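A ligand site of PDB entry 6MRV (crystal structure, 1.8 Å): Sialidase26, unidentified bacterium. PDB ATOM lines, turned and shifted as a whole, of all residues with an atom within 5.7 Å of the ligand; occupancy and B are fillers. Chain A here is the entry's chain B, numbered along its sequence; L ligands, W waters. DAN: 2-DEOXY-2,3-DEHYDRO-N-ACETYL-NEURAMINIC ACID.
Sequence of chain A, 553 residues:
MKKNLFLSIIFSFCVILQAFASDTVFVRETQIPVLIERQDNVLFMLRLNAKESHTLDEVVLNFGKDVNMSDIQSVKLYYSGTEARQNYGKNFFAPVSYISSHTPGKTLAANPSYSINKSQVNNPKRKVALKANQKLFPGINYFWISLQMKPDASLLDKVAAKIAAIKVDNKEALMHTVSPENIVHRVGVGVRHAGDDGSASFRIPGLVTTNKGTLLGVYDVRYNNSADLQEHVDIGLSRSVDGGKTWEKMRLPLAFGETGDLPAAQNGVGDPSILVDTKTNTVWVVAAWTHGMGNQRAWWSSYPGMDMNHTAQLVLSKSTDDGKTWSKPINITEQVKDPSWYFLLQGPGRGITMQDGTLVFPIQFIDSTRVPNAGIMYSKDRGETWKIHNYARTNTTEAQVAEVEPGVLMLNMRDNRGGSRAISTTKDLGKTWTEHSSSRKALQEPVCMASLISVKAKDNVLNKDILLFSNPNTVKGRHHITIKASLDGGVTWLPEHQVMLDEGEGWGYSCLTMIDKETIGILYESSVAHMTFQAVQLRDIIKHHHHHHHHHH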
ATOM      1  N   ARG A 203       7.172  -8.307  -7.391  1.00  0.00           N
ATOM      2  CA  ARG A 203       7.164  -7.844  -6.013  1.00  0.00           C
ATOM      3  C   ARG A 203       7.441  -9.009  -5.066  1.00  0.00           C
ATOM      4  O   ARG A 203       7.434 -10.171  -5.465  1.00  0.00           O
ATOM      5  CB  ARG A 203       5.843  -7.163  -5.622  1.00  0.00           C
ATOM      6  CG  ARG A 203       5.671  -5.733  -6.145  1.00  0.00           C
ATOM      7  CD  ARG A 203       4.775  -4.913  -5.222  1.00  0.00           C
ATOM      8  NE  ARG A 203       5.391  -4.796  -3.899  1.00  0.00           N
ATOM      9  CZ  ARG A 203       4.728  -4.661  -2.760  1.00  0.00           C
ATOM     10  NH1 ARG A 203       3.400  -4.621  -2.745  1.00  0.00           N
ATOM     11  NH2 ARG A 203       5.412  -4.579  -1.618  1.00  0.00           N
ATOM     12  N   ILE A 204       7.687  -8.683  -3.803  1.00  0.00           N
ATOM     13  CA  ILE A 204       7.760  -9.638  -2.699  1.00  0.00           C
ATOM     14  C   ILE A 204       8.951 -10.584  -2.843  1.00  0.00           C
ATOM     15  O   ILE A 204       8.771 -11.760  -3.221  1.00  0.00           O
ATOM     16  CB  ILE A 204       6.448 -10.440  -2.561  1.00  0.00           C
ATOM     17  CG1 ILE A 204       5.224  -9.568  -2.872  1.00  0.00           C
ATOM     18  CG2 ILE A 204       6.317 -10.979  -1.145  1.00  0.00           C
ATOM     19  CD1 ILE A 204       5.129  -8.295  -2.041  1.00  0.00           C
ATOM     20  N   ASP A 220       6.698 -12.613  -6.503  1.00  0.00           N
ATOM     21  CA  ASP A 220       5.502 -12.445  -7.319  1.00  0.00           C
ATOM     22  C   ASP A 220       5.865 -11.941  -8.707  1.00  0.00           C
ATOM     23  O   ASP A 220       6.574 -10.930  -8.845  1.00  0.00           O
ATOM     24  CB  ASP A 220       4.549 -11.419  -6.705  1.00  0.00           C
ATOM     25  CG  ASP A 220       3.836 -11.907  -5.475  1.00  0.00           C
ATOM     26  OD1 ASP A 220       4.235 -12.914  -4.870  1.00  0.00           O
ATOM     27  OD2 ASP A 220       2.843 -11.235  -5.119  1.00  0.00           O
ATOM     28  N   ARG A 222       3.580 -10.310 -11.155  1.00  0.00           N
ATOM     29  CA  ARG A 222       2.260  -9.690 -11.197  1.00  0.00           C
ATOM     30  C   ARG A 222       2.067  -9.143 -12.609  1.00  0.00           C
ATOM     31  O   ARG A 222       2.524  -8.032 -12.925  1.00  0.00           O
ATOM     32  CB  ARG A 222       2.143  -8.593 -10.131  1.00  0.00           C
ATOM     33  CG  ARG A 222       2.374  -9.096  -8.721  1.00  0.00           C
ATOM     34  CD  ARG A 222       2.175  -8.018  -7.669  1.00  0.00           C
ATOM     35  NE  ARG A 222       2.287  -8.599  -6.330  1.00  0.00           N
ATOM     36  CZ  ARG A 222       1.912  -7.998  -5.207  1.00  0.00           C
ATOM     37  NH1 ARG A 222       1.391  -6.778  -5.229  1.00  0.00           N
ATOM     38  NH2 ARG A 222       2.055  -8.627  -4.041  1.00  0.00           N
ATOM     39  N   ASP A 228      -1.956  -6.429  -5.274  1.00  0.00           N
ATOM     40  CA  ASP A 228      -1.859  -7.662  -4.512  1.00  0.00           C
ATOM     41  C   ASP A 228      -2.899  -8.673  -5.004  1.00  0.00           C
ATOM     42  O   ASP A 228      -3.829  -8.345  -5.746  1.00  0.00           O
ATOM     43  CB  ASP A 228      -2.087  -7.401  -3.015  1.00  0.00           C
ATOM     44  CG  ASP A 228      -1.107  -6.400  -2.419  1.00  0.00           C
ATOM     45  OD1 ASP A 228      -0.017  -6.180  -2.996  1.00  0.00           O
ATOM     46  OD2 ASP A 228      -1.441  -5.832  -1.350  1.00  0.00           O
ATOM     47  N   LEU A 229      -2.719  -9.930  -4.591  1.00  0.00           N
ATOM     48  CA  LEU A 229      -3.782 -10.920  -4.765  1.00  0.00           C
ATOM     49  C   LEU A 229      -5.106 -10.338  -4.287  1.00  0.00           C
ATOM     50  O   LEU A 229      -5.132  -9.539  -3.336  1.00  0.00           O
ATOM     51  CB  LEU A 229      -3.452 -12.199  -3.984  1.00  0.00           C
ATOM     52  CG  LEU A 229      -2.197 -13.002  -4.314  1.00  0.00           C
ATOM     53  CD1 LEU A 229      -2.015 -14.143  -3.324  1.00  0.00           C
ATOM     54  CD2 LEU A 229      -2.248 -13.573  -5.727  1.00  0.00           C
ATOM     55  N   ASP A 271       3.096 -13.915  -2.455  1.00  0.00           N
ATOM     56  CA  ASP A 271       3.790 -13.744  -1.184  1.00  0.00           C
ATOM     57  C   ASP A 271       4.709 -14.918  -0.847  1.00  0.00           C
ATOM     58  O   ASP A 271       4.598 -15.513   0.234  1.00  0.00           O
ATOM     59  CB  ASP A 271       2.797 -13.489  -0.058  1.00  0.00           C
ATOM     60  CG  ASP A 271       2.314 -12.050  -0.027  1.00  0.00           C
ATOM     61  OD1 ASP A 271       2.563 -11.314  -1.009  1.00  0.00           O
ATOM     62  OD2 ASP A 271       1.694 -11.657   0.995  1.00  0.00           O
ATOM     63  N   ALA A 298      -7.295 -10.343  -1.699  1.00  0.00           N
ATOM     64  CA  ALA A 298      -7.454 -11.589  -0.953  1.00  0.00           C
ATOM     65  C   ALA A 298      -7.472 -11.352   0.543  1.00  0.00           C
ATOM     66  O   ALA A 298      -8.090 -12.128   1.297  1.00  0.00           O
ATOM     67  CB  ALA A 298      -6.338 -12.560  -1.326  1.00  0.00           C
ATOM     68  N   TRP A 299      -6.817 -10.293   1.011  1.00  0.00           N
ATOM     69  CA  TRP A 299      -6.845  -9.971   2.434  1.00  0.00           C
ATOM     70  C   TRP A 299      -8.277  -9.868   2.950  1.00  0.00           C
ATOM     71  O   TRP A 299      -8.583 -10.292   4.071  1.00  0.00           O
ATOM     72  CB  TRP A 299      -6.091  -8.666   2.685  1.00  0.00           C
ATOM     73  CG  TRP A 299      -5.756  -8.432   4.121  1.00  0.00           C
ATOM     74  CD1 TRP A 299      -6.345  -7.546   4.971  1.00  0.00           C
ATOM     75  CD2 TRP A 299      -4.759  -9.115   4.894  1.00  0.00           C
ATOM     76  NE1 TRP A 299      -5.778  -7.632   6.220  1.00  0.00           N
ATOM     77  CE2 TRP A 299      -4.801  -8.597   6.198  1.00  0.00           C
ATOM     78  CE3 TRP A 299      -3.838 -10.124   4.600  1.00  0.00           C
ATOM     79  CZ2 TRP A 299      -3.947  -9.042   7.205  1.00  0.00           C
ATOM     80  CZ3 TRP A 299      -3.004 -10.576   5.602  1.00  0.00           C
ATOM     81  CH2 TRP A 299      -3.059 -10.032   6.884  1.00  0.00           C
ATOM     82  N   PHE A 343      -7.896 -16.604   6.771  1.00  0.00           N
ATOM     83  CA  PHE A 343      -6.768 -16.541   5.842  1.00  0.00           C
ATOM     84  C   PHE A 343      -5.529 -16.998   6.581  1.00  0.00           C
ATOM     85  O   PHE A 343      -5.130 -16.371   7.557  1.00  0.00           O
ATOM     86  CB  PHE A 343      -6.600 -15.102   5.321  1.00  0.00           C
ATOM     87  CG  PHE A 343      -5.714 -14.946   4.102  1.00  0.00           C
ATOM     88  CD1 PHE A 343      -4.962 -15.998   3.607  1.00  0.00           C
ATOM     89  CD2 PHE A 343      -5.630 -13.726   3.464  1.00  0.00           C
ATOM     90  CE1 PHE A 343      -4.156 -15.828   2.491  1.00  0.00           C
ATOM     91  CE2 PHE A 343      -4.840 -13.540   2.348  1.00  0.00           C
ATOM     92  CZ  PHE A 343      -4.095 -14.593   1.866  1.00  0.00           C
ATOM     93  N   LEU A 345      -1.518 -17.715   5.696  1.00  0.00           N
ATOM     94  CA  LEU A 345      -0.457 -17.724   4.697  1.00  0.00           C
ATOM     95  C   LEU A 345       0.892 -17.535   5.361  1.00  0.00           C
ATOM     96  O   LEU A 345       0.996 -17.078   6.506  1.00  0.00           O
ATOM     97  CB  LEU A 345      -0.653 -16.651   3.596  1.00  0.00           C
ATOM     98  CG  LEU A 345      -0.907 -15.166   3.858  1.00  0.00           C
ATOM     99  CD1 LEU A 345      -0.358 -14.749   5.118  1.00  0.00           C
ATOM    100  CD2 LEU A 345      -0.271 -14.285   2.798  1.00  0.00           C
ATOM    101  N   GLN A 364       1.215 -16.368   9.285  1.00  0.00           N
ATOM    102  CA  GLN A 364       0.301 -15.357   9.812  1.00  0.00           C
ATOM    103  C   GLN A 364      -1.096 -15.819   9.463  1.00  0.00           C
ATOM    104  O   GLN A 364      -1.330 -16.368   8.375  1.00  0.00           O
ATOM    105  CB  GLN A 364       0.602 -13.974   9.227  1.00  0.00           C
ATOM    106  CG  GLN A 364       0.790 -14.036   7.738  1.00  0.00           C
ATOM    107  CD  GLN A 364       1.065 -12.702   7.061  1.00  0.00           C
ATOM    108  OE1 GLN A 364       0.523 -11.673   7.451  1.00  0.00           O
ATOM    109  NE2 GLN A 364       1.872 -12.727   6.005  1.00  0.00           N
ATOM    110  N   THR A 397       1.327  -9.142  11.294  1.00  0.00           N
ATOM    111  CA  THR A 397       1.175  -9.809  10.015  1.00  0.00           C
ATOM    112  C   THR A 397       2.478 -10.469   9.573  1.00  0.00           C
ATOM    113  O   THR A 397       2.839 -11.541  10.061  1.00  0.00           O
ATOM    114  CB  THR A 397       0.691  -8.820   8.945  1.00  0.00           C
ATOM    115  OG1 THR A 397       1.576  -7.700   8.884  1.00  0.00           O
ATOM    116  CG2 THR A 397      -0.723  -8.337   9.258  1.00  0.00           C
ATOM    117  N   GLU A 398       3.195  -9.812   8.656  1.00  0.00           N
ATOM    118  CA  GLU A 398       4.404 -10.399   8.086  1.00  0.00           C
ATOM    119  C   GLU A 398       5.515 -10.459   9.116  1.00  0.00           C
ATOM    120  O   GLU A 398       5.758  -9.504   9.855  1.00  0.00           O
ATOM    121  CB  GLU A 398       4.857  -9.583   6.883  1.00  0.00           C
ATOM    122  CG  GLU A 398       3.785  -9.407   5.809  1.00  0.00           C
ATOM    123  CD  GLU A 398       4.197  -8.446   4.724  1.00  0.00           C
ATOM    124  OE1 GLU A 398       4.993  -7.515   5.013  1.00  0.00           O
ATOM    125  OE2 GLU A 398       3.732  -8.613   3.577  1.00  0.00           O
ATOM    126  N   ARG A 414       6.015  -7.392  11.608  1.00  0.00           N
ATOM    127  CA  ARG A 414       5.297  -6.200  11.183  1.00  0.00           C
ATOM    128  C   ARG A 414       4.091  -5.994  12.097  1.00  0.00           C
ATOM    129  O   ARG A 414       3.253  -6.900  12.241  1.00  0.00           O
ATOM    130  CB  ARG A 414       4.876  -6.381   9.724  1.00  0.00           C
ATOM    131  CG  ARG A 414       3.933  -5.353   9.157  1.00  0.00           C
ATOM    132  CD  ARG A 414       3.752  -5.635   7.671  1.00  0.00           C
ATOM    133  NE  ARG A 414       2.737  -4.796   7.042  1.00  0.00           N
ATOM    134  CZ  ARG A 414       2.644  -4.587   5.735  1.00  0.00           C
ATOM    135  NH1 ARG A 414       3.517  -5.142   4.900  1.00  0.00           N
ATOM    136  NH2 ARG A 414       1.684  -3.822   5.251  1.00  0.00           N
ATOM    137  N   ASN A 416       0.773  -3.761  13.211  1.00  0.00           N
ATOM    138  CA  ASN A 416      -0.205  -2.776  12.769  1.00  0.00           C
ATOM    139  C   ASN A 416      -0.371  -1.620  13.742  1.00  0.00           C
ATOM    140  O   ASN A 416      -1.013  -0.619  13.385  1.00  0.00           O
ATOM    141  CB  ASN A 416      -1.553  -3.455  12.526  1.00  0.00           C
ATOM    142  CG  ASN A 416      -1.568  -4.276  11.256  1.00  0.00           C
ATOM    143  OD1 ASN A 416      -0.874  -3.961  10.281  1.00  0.00           O
ATOM    144  ND2 ASN A 416      -2.355  -5.348  11.243  1.00  0.00           N
ATOM    145  N   VAL A 447       5.623   0.074   8.849  1.00  0.00           N
ATOM    146  CA  VAL A 447       4.673  -1.024   8.692  1.00  0.00           C
ATOM    147  C   VAL A 447       4.875  -1.602   7.299  1.00  0.00           C
ATOM    148  O   VAL A 447       4.254  -1.160   6.323  1.00  0.00           O
ATOM    149  CB  VAL A 447       3.219  -0.604   8.929  1.00  0.00           C
ATOM    150  CG1 VAL A 447       2.305  -1.812   8.824  1.00  0.00           C
ATOM    151  CG2 VAL A 447       3.072   0.035  10.315  1.00  0.00           C
ATOM    152  N   CYS A 448       5.735  -2.613   7.211  1.00  0.00           N
ATOM    153  CA  CYS A 448       6.283  -3.104   5.960  1.00  0.00           C
ATOM    154  C   CYS A 448       7.048  -4.384   6.277  1.00  0.00           C
ATOM    155  O   CYS A 448       7.467  -4.615   7.419  1.00  0.00           O
ATOM    156  CB  CYS A 448       7.178  -2.056   5.302  1.00  0.00           C
ATOM    157  SG  CYS A 448       7.922  -2.492   3.703  1.00  0.00           S
ATOM    158  N   ARG A 478       8.340   4.301   2.403  1.00  0.00           N
ATOM    159  CA  ARG A 478       9.227   3.170   2.164  1.00  0.00           C
ATOM    160  C   ARG A 478      10.424   3.669   1.352  1.00  0.00           C
ATOM    161  O   ARG A 478      10.424   3.630   0.117  1.00  0.00           O
ATOM    162  CB  ARG A 478       8.489   2.020   1.477  1.00  0.00           C
ATOM    163  CG  ARG A 478       7.371   1.478   2.343  1.00  0.00           C
ATOM    164  CD  ARG A 478       6.659   0.290   1.719  1.00  0.00           C
ATOM    165  NE  ARG A 478       5.564  -0.160   2.578  1.00  0.00           N
ATOM    166  CZ  ARG A 478       4.715  -1.143   2.264  1.00  0.00           C
ATOM    167  NH1 ARG A 478       4.837  -1.780   1.108  1.00  0.00           N
ATOM    168  NH2 ARG A 478       3.748  -1.466   3.113  1.00  0.00           N
ATOM    169  N   TRP A 507       8.783   0.021  -3.043  1.00  0.00           N
ATOM    170  CA  TRP A 507       7.770  -0.803  -2.399  1.00  0.00           C
ATOM    171  C   TRP A 507       8.262  -1.417  -1.089  1.00  0.00           C
ATOM    172  O   TRP A 507       7.444  -1.919  -0.310  1.00  0.00           O
ATOM    173  CB  TRP A 507       7.288  -1.920  -3.339  1.00  0.00           C
ATOM    174  CG  TRP A 507       6.253  -1.496  -4.374  1.00  0.00           C
ATOM    175  CD1 TRP A 507       6.420  -1.437  -5.734  1.00  0.00           C
ATOM    176  CD2 TRP A 507       4.890  -1.087  -4.131  1.00  0.00           C
ATOM    177  NE1 TRP A 507       5.253  -1.019  -6.346  1.00  0.00           N
ATOM    178  CE2 TRP A 507       4.301  -0.796  -5.376  1.00  0.00           C
ATOM    179  CE3 TRP A 507       4.122  -0.943  -2.966  1.00  0.00           C
ATOM    180  CZ2 TRP A 507       2.982  -0.374  -5.502  1.00  0.00           C
ATOM    181  CZ3 TRP A 507       2.803  -0.521  -3.091  1.00  0.00           C
ATOM    182  CH2 TRP A 507       2.247  -0.241  -4.350  1.00  0.00           C
ATOM    183  N   TYR A 509      10.026  -3.976   0.325  1.00  0.00           N
ATOM    184  CA  TYR A 509      10.307  -5.330   0.818  1.00  0.00           C
ATOM    185  C   TYR A 509      11.740  -5.744   0.492  1.00  0.00           C
ATOM    186  O   TYR A 509      12.343  -5.268  -0.471  1.00  0.00           O
ATOM    187  CB  TYR A 509       9.335  -6.341   0.191  1.00  0.00           C
ATOM    188  CG  TYR A 509       7.934  -6.358   0.771  1.00  0.00           C
ATOM    189  CD1 TYR A 509       7.247  -7.554   0.892  1.00  0.00           C
ATOM    190  CD2 TYR A 509       7.297  -5.191   1.177  1.00  0.00           C
ATOM    191  CE1 TYR A 509       5.969  -7.600   1.404  1.00  0.00           C
ATOM    192  CE2 TYR A 509       6.018  -5.226   1.697  1.00  0.00           C
ATOM    193  CZ  TYR A 509       5.364  -6.433   1.804  1.00  0.00           C
ATOM    194  OH  TYR A 509       4.096  -6.507   2.319  1.00  0.00           O
HETATM  195  C1  DAN L   1       2.353  -4.321   1.152  1.00  0.00           C
HETATM  196  C2  DAN L   1       1.684  -5.666   1.087  1.00  0.00           C
HETATM  197  C3  DAN L   1       2.138  -6.768  -0.015  1.00  0.00           C
HETATM  198  C4  DAN L   1       1.686  -8.016   0.176  1.00  0.00           C
HETATM  199  C5  DAN L   1       0.258  -8.016   1.045  1.00  0.00           C
HETATM  200  C6  DAN L   1       0.434  -7.545   2.298  1.00  0.00           C
HETATM  201  C7  DAN L   1      -0.870  -7.466   3.114  1.00  0.00           C
HETATM  202  C8  DAN L   1      -0.649  -6.674   4.352  1.00  0.00           C
HETATM  203  C9  DAN L   1      -1.860  -6.751   5.319  1.00  0.00           C
HETATM  204  C10 DAN L   1      -1.594  -9.784   0.835  1.00  0.00           C
HETATM  205  C11 DAN L   1      -2.037 -11.271   0.814  1.00  0.00           C
HETATM  206  N5  DAN L   1      -0.171  -9.476   1.028  1.00  0.00           N
HETATM  207  O1A DAN L   1       3.145  -3.936   0.231  1.00  0.00           O
HETATM  208  O1B DAN L   1       2.100  -3.548   2.197  1.00  0.00           O
HETATM  209  O4  DAN L   1       1.453  -8.675  -1.070  1.00  0.00           O
HETATM  210  O6  DAN L   1       1.028  -6.066   2.263  1.00  0.00           O
HETATM  211  O7  DAN L   1      -1.867  -6.826   2.327  1.00  0.00           O
HETATM  212  O8  DAN L   1       0.491  -7.158   5.040  1.00  0.00           O
HETATM  213  O9  DAN L   1      -1.769  -5.711   6.275  1.00  0.00           O
HETATM  214  O10 DAN L   1      -2.377  -8.896   0.702  1.00  0.00           O
HETATM  215  O   HOH W   1      -3.496  -5.885   8.667  1.00  0.00           O
HETATM  216  O   HOH W   2      -0.821 -10.191  -2.405  1.00  0.00           O
HETATM  217  O   HOH W   3       0.155  -5.205   8.169  1.00  0.00           O
HETATM  218  O   HOH W   4       0.439  -9.614   5.251  1.00  0.00           O
HETATM  219  O   HOH W   5      -4.666  -8.952  -0.488  1.00  0.00           O
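Merely in contact with the ligand: Ile 204, Trp 299, Phe 343 and Glu 398. Hydrophobic or aromatic side chains that line the ligand: Ile 204, Trp 299, Phe 343 and Tyr 509. Of the 21 residues printed, 11 come within 4 Å of the ligand. Along chain A the residues within 4 Å of the ligand span positions 203 to 509. The nearest printed residue that does not touch the ligand is Leu 345 (4.02 Å).
Water W4 lies within hydrogen-bond range of O8 of the ligand and OE1 of Gln 364. Water W5 lies within hydrogen-bond range of an oxygen (O10) of the ligand (2.6 Å), the backbone carbonyl oxygen (O) of Leu 229 (2.9 Å), the backbone NH (N) of Trp 299 (2.9 Å) and the backbone NH (N) of Ala 298 (3.2 Å). Water W3 lies within hydrogen-bond range of the side-chain amide oxygen (OD1) of Asn 416 (2.7 Å), an oxygen (O9) of the ligand (2.7 Å), the guanidinium group (NE) of Arg 414 (2.8 Å) and the side-chain hydroxyl (OG1) of Thr 397 (3.0 Å). Water W1 bridges the side-chain amide nitrogen (ND2) of Asn 416 and an oxygen (O9) of the ligand. Water W2 bridges the backbone NH (N) of Leu 229 (2.9 Å) and an oxygen (O4) of the ligand (3.0 Å).
NH2 of Arg 203 is in salt-bridge range of O1A of the ligand (3.0 Å). The guanidinium group (NH2) of Arg 478 lies within salt-bridge range of an oxygen (O1B) of the ligand, 2.8 Å away. An oxygen (O6) of the ligand sits close to the side-chain hydroxyl (OH) of Tyr 509, 3.1 Å away. The side-chain carboxylate (OD1) of Asp 228 is in hydrogen-bond range of an oxygen (O4) of the ligand (3.5 Å). O4 of the ligand sits at hydrogen-bond distance from OD1 of Asp 271, 2.9 Å away. The guanidinium group (NH2) of Arg 414 is in salt-bridge range of an oxygen (O1B) of the ligand, 3.1 Å away. An oxygen (O4) of the ligand is in hydrogen-bond range of the guanidinium group (NH2) of Arg 222.
The side-chain hydroxyl (OH) of Tyr 509 lies within hydrogen-bond range of the side-chain carboxylate (OE2) of Glu 398, 2.5 Å away. The side-chain carboxylate (OD1) of Asp 220 is in hydrogen-bond range of the backbone NH (N) of Asp 271. NH1 of Arg 203 lies within salt-bridge range of OD1 of Asp 228, 3.8 Å away. The backbone carbonyl oxygen (O) of Arg 203 lies within hydrogen-bond range of the backbone NH (N) of Asp 220. NH2 of Arg 478 lies within hydrogen-bond range of O of Val 447. The guanidinium group (NE) of Arg 478 is in hydrogen-bond range of the side-chain sulfur (SG) of Cys 448, 3.5 Å away. The guanidinium group (NH1) of Arg 478 sits at hydrogen-bond distance from the backbone carbonyl oxygen (O) of Trp 507, 3.0 Å away. The guanidinium group (NH1) of Arg 222 lies within salt-bridge range of the side-chain carboxylate (OD1) of Asp 228, at 2.7 Å.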
